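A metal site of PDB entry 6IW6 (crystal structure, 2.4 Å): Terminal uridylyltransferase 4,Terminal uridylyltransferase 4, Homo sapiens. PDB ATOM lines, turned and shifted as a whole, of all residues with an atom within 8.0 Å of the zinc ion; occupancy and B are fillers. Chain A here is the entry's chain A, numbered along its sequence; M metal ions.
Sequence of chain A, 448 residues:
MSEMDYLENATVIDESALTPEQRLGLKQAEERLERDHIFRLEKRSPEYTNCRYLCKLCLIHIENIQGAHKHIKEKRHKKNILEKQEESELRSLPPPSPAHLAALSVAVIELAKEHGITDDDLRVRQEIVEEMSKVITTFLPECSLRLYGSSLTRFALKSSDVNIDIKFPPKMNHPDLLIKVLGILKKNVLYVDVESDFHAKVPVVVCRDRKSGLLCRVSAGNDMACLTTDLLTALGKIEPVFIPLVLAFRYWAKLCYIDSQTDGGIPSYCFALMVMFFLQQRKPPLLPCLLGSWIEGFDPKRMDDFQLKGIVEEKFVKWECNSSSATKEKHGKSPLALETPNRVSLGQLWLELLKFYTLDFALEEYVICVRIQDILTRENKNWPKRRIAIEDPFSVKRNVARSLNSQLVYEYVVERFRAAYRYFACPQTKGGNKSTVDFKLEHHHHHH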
ATOM      1  N   ASP A  36       0.659 -19.463 -31.472  1.00  0.00           N
ATOM      2  CA  ASP A  36       1.321 -20.755 -31.621  1.00  0.00           C
ATOM      3  C   ASP A  36       1.529 -21.452 -30.283  1.00  0.00           C
ATOM      4  O   ASP A  36       2.412 -22.311 -30.173  1.00  0.00           O
ATOM      5  CB  ASP A  36       2.649 -20.602 -32.359  1.00  0.00           C
ATOM      6  CG  ASP A  36       2.461 -20.424 -33.853  1.00  0.00           C
ATOM      7  OD1 ASP A  36       1.936 -21.354 -34.506  1.00  0.00           O
ATOM      8  OD2 ASP A  36       2.840 -19.363 -34.377  1.00  0.00           O
ATOM      9  N   HIS A  37       0.732 -21.092 -29.260  1.00  0.00           N
ATOM     10  CA  HIS A  37       0.683 -21.742 -27.946  1.00  0.00           C
ATOM     11  C   HIS A  37       1.835 -21.353 -27.018  1.00  0.00           C
ATOM     12  O   HIS A  37       2.101 -22.064 -26.040  1.00  0.00           O
ATOM     13  CB  HIS A  37       0.646 -23.271 -28.048  1.00  0.00           C
ATOM     14  CG  HIS A  37      -0.355 -23.791 -29.042  1.00  0.00           C
ATOM     15  ND1 HIS A  37      -1.688 -23.974 -28.737  1.00  0.00           N
ATOM     16  CD2 HIS A  37      -0.210 -24.172 -30.328  1.00  0.00           C
ATOM     17  CE1 HIS A  37      -2.316 -24.446 -29.797  1.00  0.00           C
ATOM     18  NE2 HIS A  37      -1.443 -24.564 -30.779  1.00  0.00           N
ATOM     19  N   ILE A  38       2.516 -20.237 -27.280  1.00  0.00           N
ATOM     20  CA  ILE A  38       3.697 -19.844 -26.513  1.00  0.00           C
ATOM     21  C   ILE A  38       3.363 -18.615 -25.679  1.00  0.00           C
ATOM     22  O   ILE A  38       2.916 -17.594 -26.215  1.00  0.00           O
ATOM     23  CB  ILE A  38       4.887 -19.579 -27.452  1.00  0.00           C
ATOM     24  CG1 ILE A  38       5.290 -20.899 -28.120  1.00  0.00           C
ATOM     25  CG2 ILE A  38       6.050 -18.951 -26.703  1.00  0.00           C
ATOM     26  CD1 ILE A  38       6.181 -20.719 -29.323  1.00  0.00           C
ATOM     27  N   LEU A  54       6.740 -20.508 -21.945  1.00  0.00           N
ATOM     28  CA  LEU A  54       6.272 -21.892 -21.946  1.00  0.00           C
ATOM     29  C   LEU A  54       5.478 -22.117 -23.222  1.00  0.00           C
ATOM     30  O   LEU A  54       4.607 -21.317 -23.568  1.00  0.00           O
ATOM     31  CB  LEU A  54       5.407 -22.185 -20.719  1.00  0.00           C
ATOM     32  CG  LEU A  54       5.054 -23.644 -20.375  1.00  0.00           C
ATOM     33  CD1 LEU A  54       3.744 -24.060 -21.005  1.00  0.00           C
ATOM     34  CD2 LEU A  54       6.158 -24.581 -20.812  1.00  0.00           C
ATOM     35  N   CYS A  55       5.808 -23.190 -23.939  1.00  0.00           N
ATOM     36  CA  CYS A  55       4.971 -23.701 -25.005  1.00  0.00           C
ATOM     37  C   CYS A  55       4.025 -24.723 -24.400  1.00  0.00           C
ATOM     38  O   CYS A  55       4.462 -25.788 -23.921  1.00  0.00           O
ATOM     39  CB  CYS A  55       5.787 -24.320 -26.137  1.00  0.00           C
ATOM     40  SG  CYS A  55       4.693 -25.084 -27.359  1.00  0.00           S
ATOM     41  N   LYS A  56       2.717 -24.377 -24.387  1.00  0.00           N
ATOM     42  CA  LYS A  56       1.693 -25.233 -23.797  1.00  0.00           C
ATOM     43  C   LYS A  56       1.453 -26.474 -24.643  1.00  0.00           C
ATOM     44  O   LYS A  56       1.025 -27.504 -24.120  1.00  0.00           O
ATOM     45  CB  LYS A  56       0.388 -24.443 -23.622  1.00  0.00           C
ATOM     46  CG  LYS A  56       0.531 -23.155 -22.837  1.00  0.00           C
ATOM     47  CD  LYS A  56      -0.814 -22.487 -22.588  1.00  0.00           C
ATOM     48  CE  LYS A  56      -1.735 -23.377 -21.768  1.00  0.00           C
ATOM     49  NZ  LYS A  56      -3.000 -22.668 -21.381  1.00  0.00           N
ATOM     50  N   LEU A  57       1.683 -26.381 -25.958  1.00  0.00           N
ATOM     51  CA  LEU A  57       1.584 -27.562 -26.803  1.00  0.00           C
ATOM     52  C   LEU A  57       2.619 -28.595 -26.385  1.00  0.00           C
ATOM     53  O   LEU A  57       2.270 -29.698 -25.939  1.00  0.00           O
ATOM     54  CB  LEU A  57       1.788 -27.168 -28.269  1.00  0.00           C
ATOM     55  CG  LEU A  57       1.792 -28.277 -29.324  1.00  0.00           C
ATOM     56  CD1 LEU A  57       0.442 -28.966 -29.357  1.00  0.00           C
ATOM     57  CD2 LEU A  57       2.163 -27.754 -30.711  1.00  0.00           C
ATOM     58  N   CYS A  58       3.899 -28.256 -26.518  1.00  0.00           N
ATOM     59  CA  CYS A  58       4.968 -29.196 -26.229  1.00  0.00           C
ATOM     60  C   CYS A  58       5.318 -29.280 -24.748  1.00  0.00           C
ATOM     61  O   CYS A  58       6.131 -30.123 -24.360  1.00  0.00           O
ATOM     62  CB  CYS A  58       6.225 -28.819 -27.026  1.00  0.00           C
ATOM     63  SG  CYS A  58       5.981 -28.654 -28.796  1.00  0.00           S
ATOM     64  N   LEU A  59       4.704 -28.439 -23.913  1.00  0.00           N
ATOM     65  CA  LEU A  59       5.119 -28.280 -22.517  1.00  0.00           C
ATOM     66  C   LEU A  59       6.631 -28.069 -22.430  1.00  0.00           C
ATOM     67  O   LEU A  59       7.335 -28.766 -21.695  1.00  0.00           O
ATOM     68  CB  LEU A  59       4.666 -29.468 -21.658  1.00  0.00           C
ATOM     69  CG  LEU A  59       3.166 -29.725 -21.449  1.00  0.00           C
ATOM     70  CD1 LEU A  59       2.926 -31.031 -20.701  1.00  0.00           C
ATOM     71  CD2 LEU A  59       2.465 -28.566 -20.747  1.00  0.00           C
ATOM     72  N   ILE A  60       7.126 -27.111 -23.200  1.00  0.00           N
ATOM     73  CA  ILE A  60       8.569 -26.905 -23.317  1.00  0.00           C
ATOM     74  C   ILE A  60       8.913 -25.491 -22.868  1.00  0.00           C
ATOM     75  O   ILE A  60       8.251 -24.526 -23.268  1.00  0.00           O
ATOM     76  CB  ILE A  60       9.083 -27.162 -24.750  1.00  0.00           C
ATOM     77  CG1 ILE A  60       8.979 -28.647 -25.066  1.00  0.00           C
ATOM     78  CG2 ILE A  60      10.538 -26.738 -24.880  1.00  0.00           C
ATOM     79  CD1 ILE A  60       9.536 -29.523 -23.974  1.00  0.00           C
ATOM     80  N   ILE A  62      11.037 -22.279 -23.190  1.00  0.00           N
ATOM     81  CA  ILE A  62      11.769 -21.546 -24.214  1.00  0.00           C
ATOM     82  C   ILE A  62      12.291 -20.264 -23.592  1.00  0.00           C
ATOM     83  O   ILE A  62      11.587 -19.609 -22.810  1.00  0.00           O
ATOM     84  CB  ILE A  62      10.873 -21.262 -25.440  1.00  0.00           C
ATOM     85  CG1 ILE A  62      10.422 -22.581 -26.086  1.00  0.00           C
ATOM     86  CG2 ILE A  62      11.612 -20.392 -26.441  1.00  0.00           C
ATOM     87  CD1 ILE A  62       9.199 -22.453 -26.963  1.00  0.00           C
ATOM     88  N   ALA A  68      11.646 -18.915 -29.452  1.00  0.00           N
ATOM     89  CA  ALA A  68      10.259 -19.325 -29.641  1.00  0.00           C
ATOM     90  C   ALA A  68       9.938 -19.439 -31.128  1.00  0.00           C
ATOM     91  O   ALA A  68       9.258 -20.395 -31.541  1.00  0.00           O
ATOM     92  CB  ALA A  68       9.319 -18.321 -28.956  1.00  0.00           C
ATOM     93  N   HIS A  71      11.452 -22.543 -32.374  1.00  0.00           N
ATOM     94  CA  HIS A  71      10.791 -23.734 -31.845  1.00  0.00           C
ATOM     95  C   HIS A  71       9.485 -24.022 -32.593  1.00  0.00           C
ATOM     96  O   HIS A  71       9.159 -25.182 -32.847  1.00  0.00           O
ATOM     97  CB  HIS A  71      10.530 -23.557 -30.351  1.00  0.00           C
ATOM     98  CG  HIS A  71       9.629 -24.596 -29.759  1.00  0.00           C
ATOM     99  ND1 HIS A  71      10.091 -25.782 -29.235  1.00  0.00           N
ATOM    100  CD2 HIS A  71       8.280 -24.623 -29.595  1.00  0.00           C
ATOM    101  CE1 HIS A  71       9.080 -26.491 -28.788  1.00  0.00           C
ATOM    102  NE2 HIS A  71       7.966 -25.809 -28.997  1.00  0.00           N
ATOM    103  N   ILE A  72       8.732 -22.961 -32.917  1.00  0.00           N
ATOM    104  CA  ILE A  72       7.478 -23.122 -33.663  1.00  0.00           C
ATOM    105  C   ILE A  72       7.691 -23.965 -34.914  1.00  0.00           C
ATOM    106  O   ILE A  72       6.839 -24.785 -35.280  1.00  0.00           O
ATOM    107  CB  ILE A  72       6.906 -21.736 -34.016  1.00  0.00           C
ATOM    108  CG1 ILE A  72       6.284 -21.076 -32.785  1.00  0.00           C
ATOM    109  CG2 ILE A  72       5.892 -21.831 -35.138  1.00  0.00           C
ATOM    110  CD1 ILE A  72       5.942 -19.617 -33.015  1.00  0.00           C
ATOM    111  N   LYS A  73       8.829 -23.794 -35.576  1.00  0.00           N
ATOM    112  CA  LYS A  73       9.095 -24.431 -36.847  1.00  0.00           C
ATOM    113  C   LYS A  73       9.969 -25.672 -36.732  1.00  0.00           C
ATOM    114  O   LYS A  73      10.411 -26.196 -37.756  1.00  0.00           O
ATOM    115  CB  LYS A  73       9.724 -23.425 -37.815  1.00  0.00           C
ATOM    116  CG  LYS A  73       8.791 -22.302 -38.223  1.00  0.00           C
ATOM    117  CD  LYS A  73       7.745 -22.805 -39.204  1.00  0.00           C
ATOM    118  CE  LYS A  73       8.401 -23.204 -40.525  1.00  0.00           C
ATOM    119  NZ  LYS A  73       7.504 -24.034 -41.381  1.00  0.00           N
ATOM    120  N   GLU A  74      10.224 -26.158 -35.523  1.00  0.00           N
ATOM    121  CA  GLU A  74      11.111 -27.289 -35.315  1.00  0.00           C
ATOM    122  C   GLU A  74      10.310 -28.599 -35.238  1.00  0.00           C
ATOM    123  O   GLU A  74       9.089 -28.630 -35.453  1.00  0.00           O
ATOM    124  CB  GLU A  74      11.968 -27.058 -34.076  1.00  0.00           C
ATOM    125  CG  GLU A  74      13.343 -26.477 -34.404  1.00  0.00           C
ATOM    126  CD  GLU A  74      13.996 -25.771 -33.229  1.00  0.00           C
ATOM    127  OE1 GLU A  74      14.963 -25.003 -33.447  1.00  0.00           O
ATOM    128  OE2 GLU A  74      13.541 -25.991 -32.078  1.00  0.00           O
ATOM    129  N   LYS A  75      10.999 -29.692 -34.917  1.00  0.00           N
ATOM    130  CA  LYS A  75      10.400 -31.024 -35.036  1.00  0.00           C
ATOM    131  C   LYS A  75       9.299 -31.244 -34.000  1.00  0.00           C
ATOM    132  O   LYS A  75       8.183 -31.626 -34.351  1.00  0.00           O
ATOM    133  CB  LYS A  75      11.472 -32.097 -34.898  1.00  0.00           C
ATOM    134  CG  LYS A  75      12.180 -32.455 -36.188  1.00  0.00           C
ATOM    135  CD  LYS A  75      13.267 -33.497 -35.949  1.00  0.00           C
ATOM    136  CE  LYS A  75      14.004 -33.841 -37.245  1.00  0.00           C
ATOM    137  NZ  LYS A  75      13.129 -34.567 -38.203  1.00  0.00           N
ATOM    138  N   ARG A  76       9.618 -31.030 -32.729  1.00  0.00           N
ATOM    139  CA  ARG A  76       8.679 -31.345 -31.652  1.00  0.00           C
ATOM    140  C   ARG A  76       7.354 -30.608 -31.858  1.00  0.00           C
ATOM    141  O   ARG A  76       6.276 -31.211 -31.779  1.00  0.00           O
ATOM    142  CB  ARG A  76       9.286 -30.990 -30.303  1.00  0.00           C
ATOM    143  CG  ARG A  76       8.920 -31.945 -29.169  1.00  0.00           C
ATOM    144  CD  ARG A  76       9.772 -31.677 -27.935  1.00  0.00           C
ATOM    145  NE  ARG A  76       9.790 -32.824 -27.026  1.00  0.00           N
ATOM    146  CZ  ARG A  76      10.551 -33.902 -27.211  1.00  0.00           C
ATOM    147  NH1 ARG A  76      11.358 -33.982 -28.270  1.00  0.00           N
ATOM    148  NH2 ARG A  76      10.514 -34.896 -26.336  1.00  0.00           N
ATOM    149  N   HIS A  77       7.421 -29.303 -32.136  1.00  0.00           N
ATOM    150  CA  HIS A  77       6.203 -28.513 -32.284  1.00  0.00           C
ATOM    151  C   HIS A  77       5.398 -28.956 -33.503  1.00  0.00           C
ATOM    152  O   HIS A  77       4.165 -29.045 -33.444  1.00  0.00           O
ATOM    153  CB  HIS A  77       6.562 -27.034 -32.392  1.00  0.00           C
ATOM    154  CG  HIS A  77       5.403 -26.118 -32.179  1.00  0.00           C
ATOM    155  ND1 HIS A  77       4.929 -25.803 -30.914  1.00  0.00           N
ATOM    156  CD2 HIS A  77       4.626 -25.450 -33.057  1.00  0.00           C
ATOM    157  CE1 HIS A  77       3.906 -24.981 -31.031  1.00  0.00           C
ATOM    158  NE2 HIS A  77       3.703 -24.745 -32.318  1.00  0.00           N
ATOM    159  N   LYS A  78       6.074 -29.226 -34.624  1.00  0.00           N
ATOM    160  CA  LYS A  78       5.365 -29.692 -35.818  1.00  0.00           C
ATOM    161  C   LYS A  78       4.655 -31.011 -35.553  1.00  0.00           C
ATOM    162  O   LYS A  78       3.474 -31.180 -35.876  1.00  0.00           O
ATOM    163  CB  LYS A  78       6.349 -29.820 -36.980  1.00  0.00           C
ATOM    164  CG  LYS A  78       6.631 -28.517 -37.712  1.00  0.00           C
ATOM    165  CD  LYS A  78       7.507 -28.762 -38.939  1.00  0.00           C
ATOM    166  CE  LYS A  78       7.461 -27.590 -39.917  1.00  0.00           C
ATOM    167  NZ  LYS A  78       6.131 -27.457 -40.578  1.00  0.00           N
ATOM    168  N   ASN A  80       3.660 -32.242 -32.738  1.00  0.00           N
ATOM    169  CA  ASN A  80       2.537 -32.097 -31.816  1.00  0.00           C
ATOM    170  C   ASN A  80       1.347 -31.447 -32.489  1.00  0.00           C
ATOM    171  O   ASN A  80       0.197 -31.832 -32.244  1.00  0.00           O
ATOM    172  CB  ASN A  80       2.964 -31.311 -30.581  1.00  0.00           C
ATOM    173  CG  ASN A  80       3.808 -32.127 -29.638  1.00  0.00           C
ATOM    174  OD1 ASN A  80       4.456 -33.089 -30.041  1.00  0.00           O
ATOM    175  ND2 ASN A  80       3.778 -31.769 -28.357  1.00  0.00           N
ATOM    176  N   ILE A  81       1.593 -30.446 -33.346  1.00  0.00           N
ATOM    177  CA  ILE A  81       0.527 -29.864 -34.143  1.00  0.00           C
ATOM    178  C   ILE A  81      -0.189 -30.959 -34.935  1.00  0.00           C
ATOM    179  O   ILE A  81      -1.428 -31.035 -34.963  1.00  0.00           O
ATOM    180  CB  ILE A  81       1.088 -28.764 -35.074  1.00  0.00           C
ATOM    181  CG1 ILE A  81       1.401 -27.496 -34.289  1.00  0.00           C
ATOM    182  CG2 ILE A  81       0.128 -28.487 -36.220  1.00  0.00           C
ATOM    183  CD1 ILE A  81       0.167 -26.771 -33.792  1.00  0.00           C
HETATM  184 ZN    ZN M   1       5.751 -26.251 -29.074  1.00  0.00          ZN
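The backbone carbonyl oxygen (O) of Ile 60 is in hydrogen-bond range of the backbone NH (N) of Cys 55.
The side-chain sulfur (SG) of Cys 55 lies close to the backbone NH (N) of Leu 57, 3.6 Å away.
A ring nitrogen (NE2) of His 77 sits close to the backbone carbonyl oxygen (O) of Asp 36, at 3.5 Å.
Four residues have an atom within 4 Å of the zinc ion: Cys 55, Cys 58, His 71 and His 77.
The nearest printed residue that does not touch the zinc ion is Leu 57 (4.1 Å).
The zinc ion is bound by a ring nitrogen (ND1) of His 77 (2.1 Å), a ring nitrogen (NE2) of His 71 (2.3 Å), the side-chain sulfur of Cys 55 (2.3 Å) and the side-chain sulfur of Cys 58 (2.4 Å).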
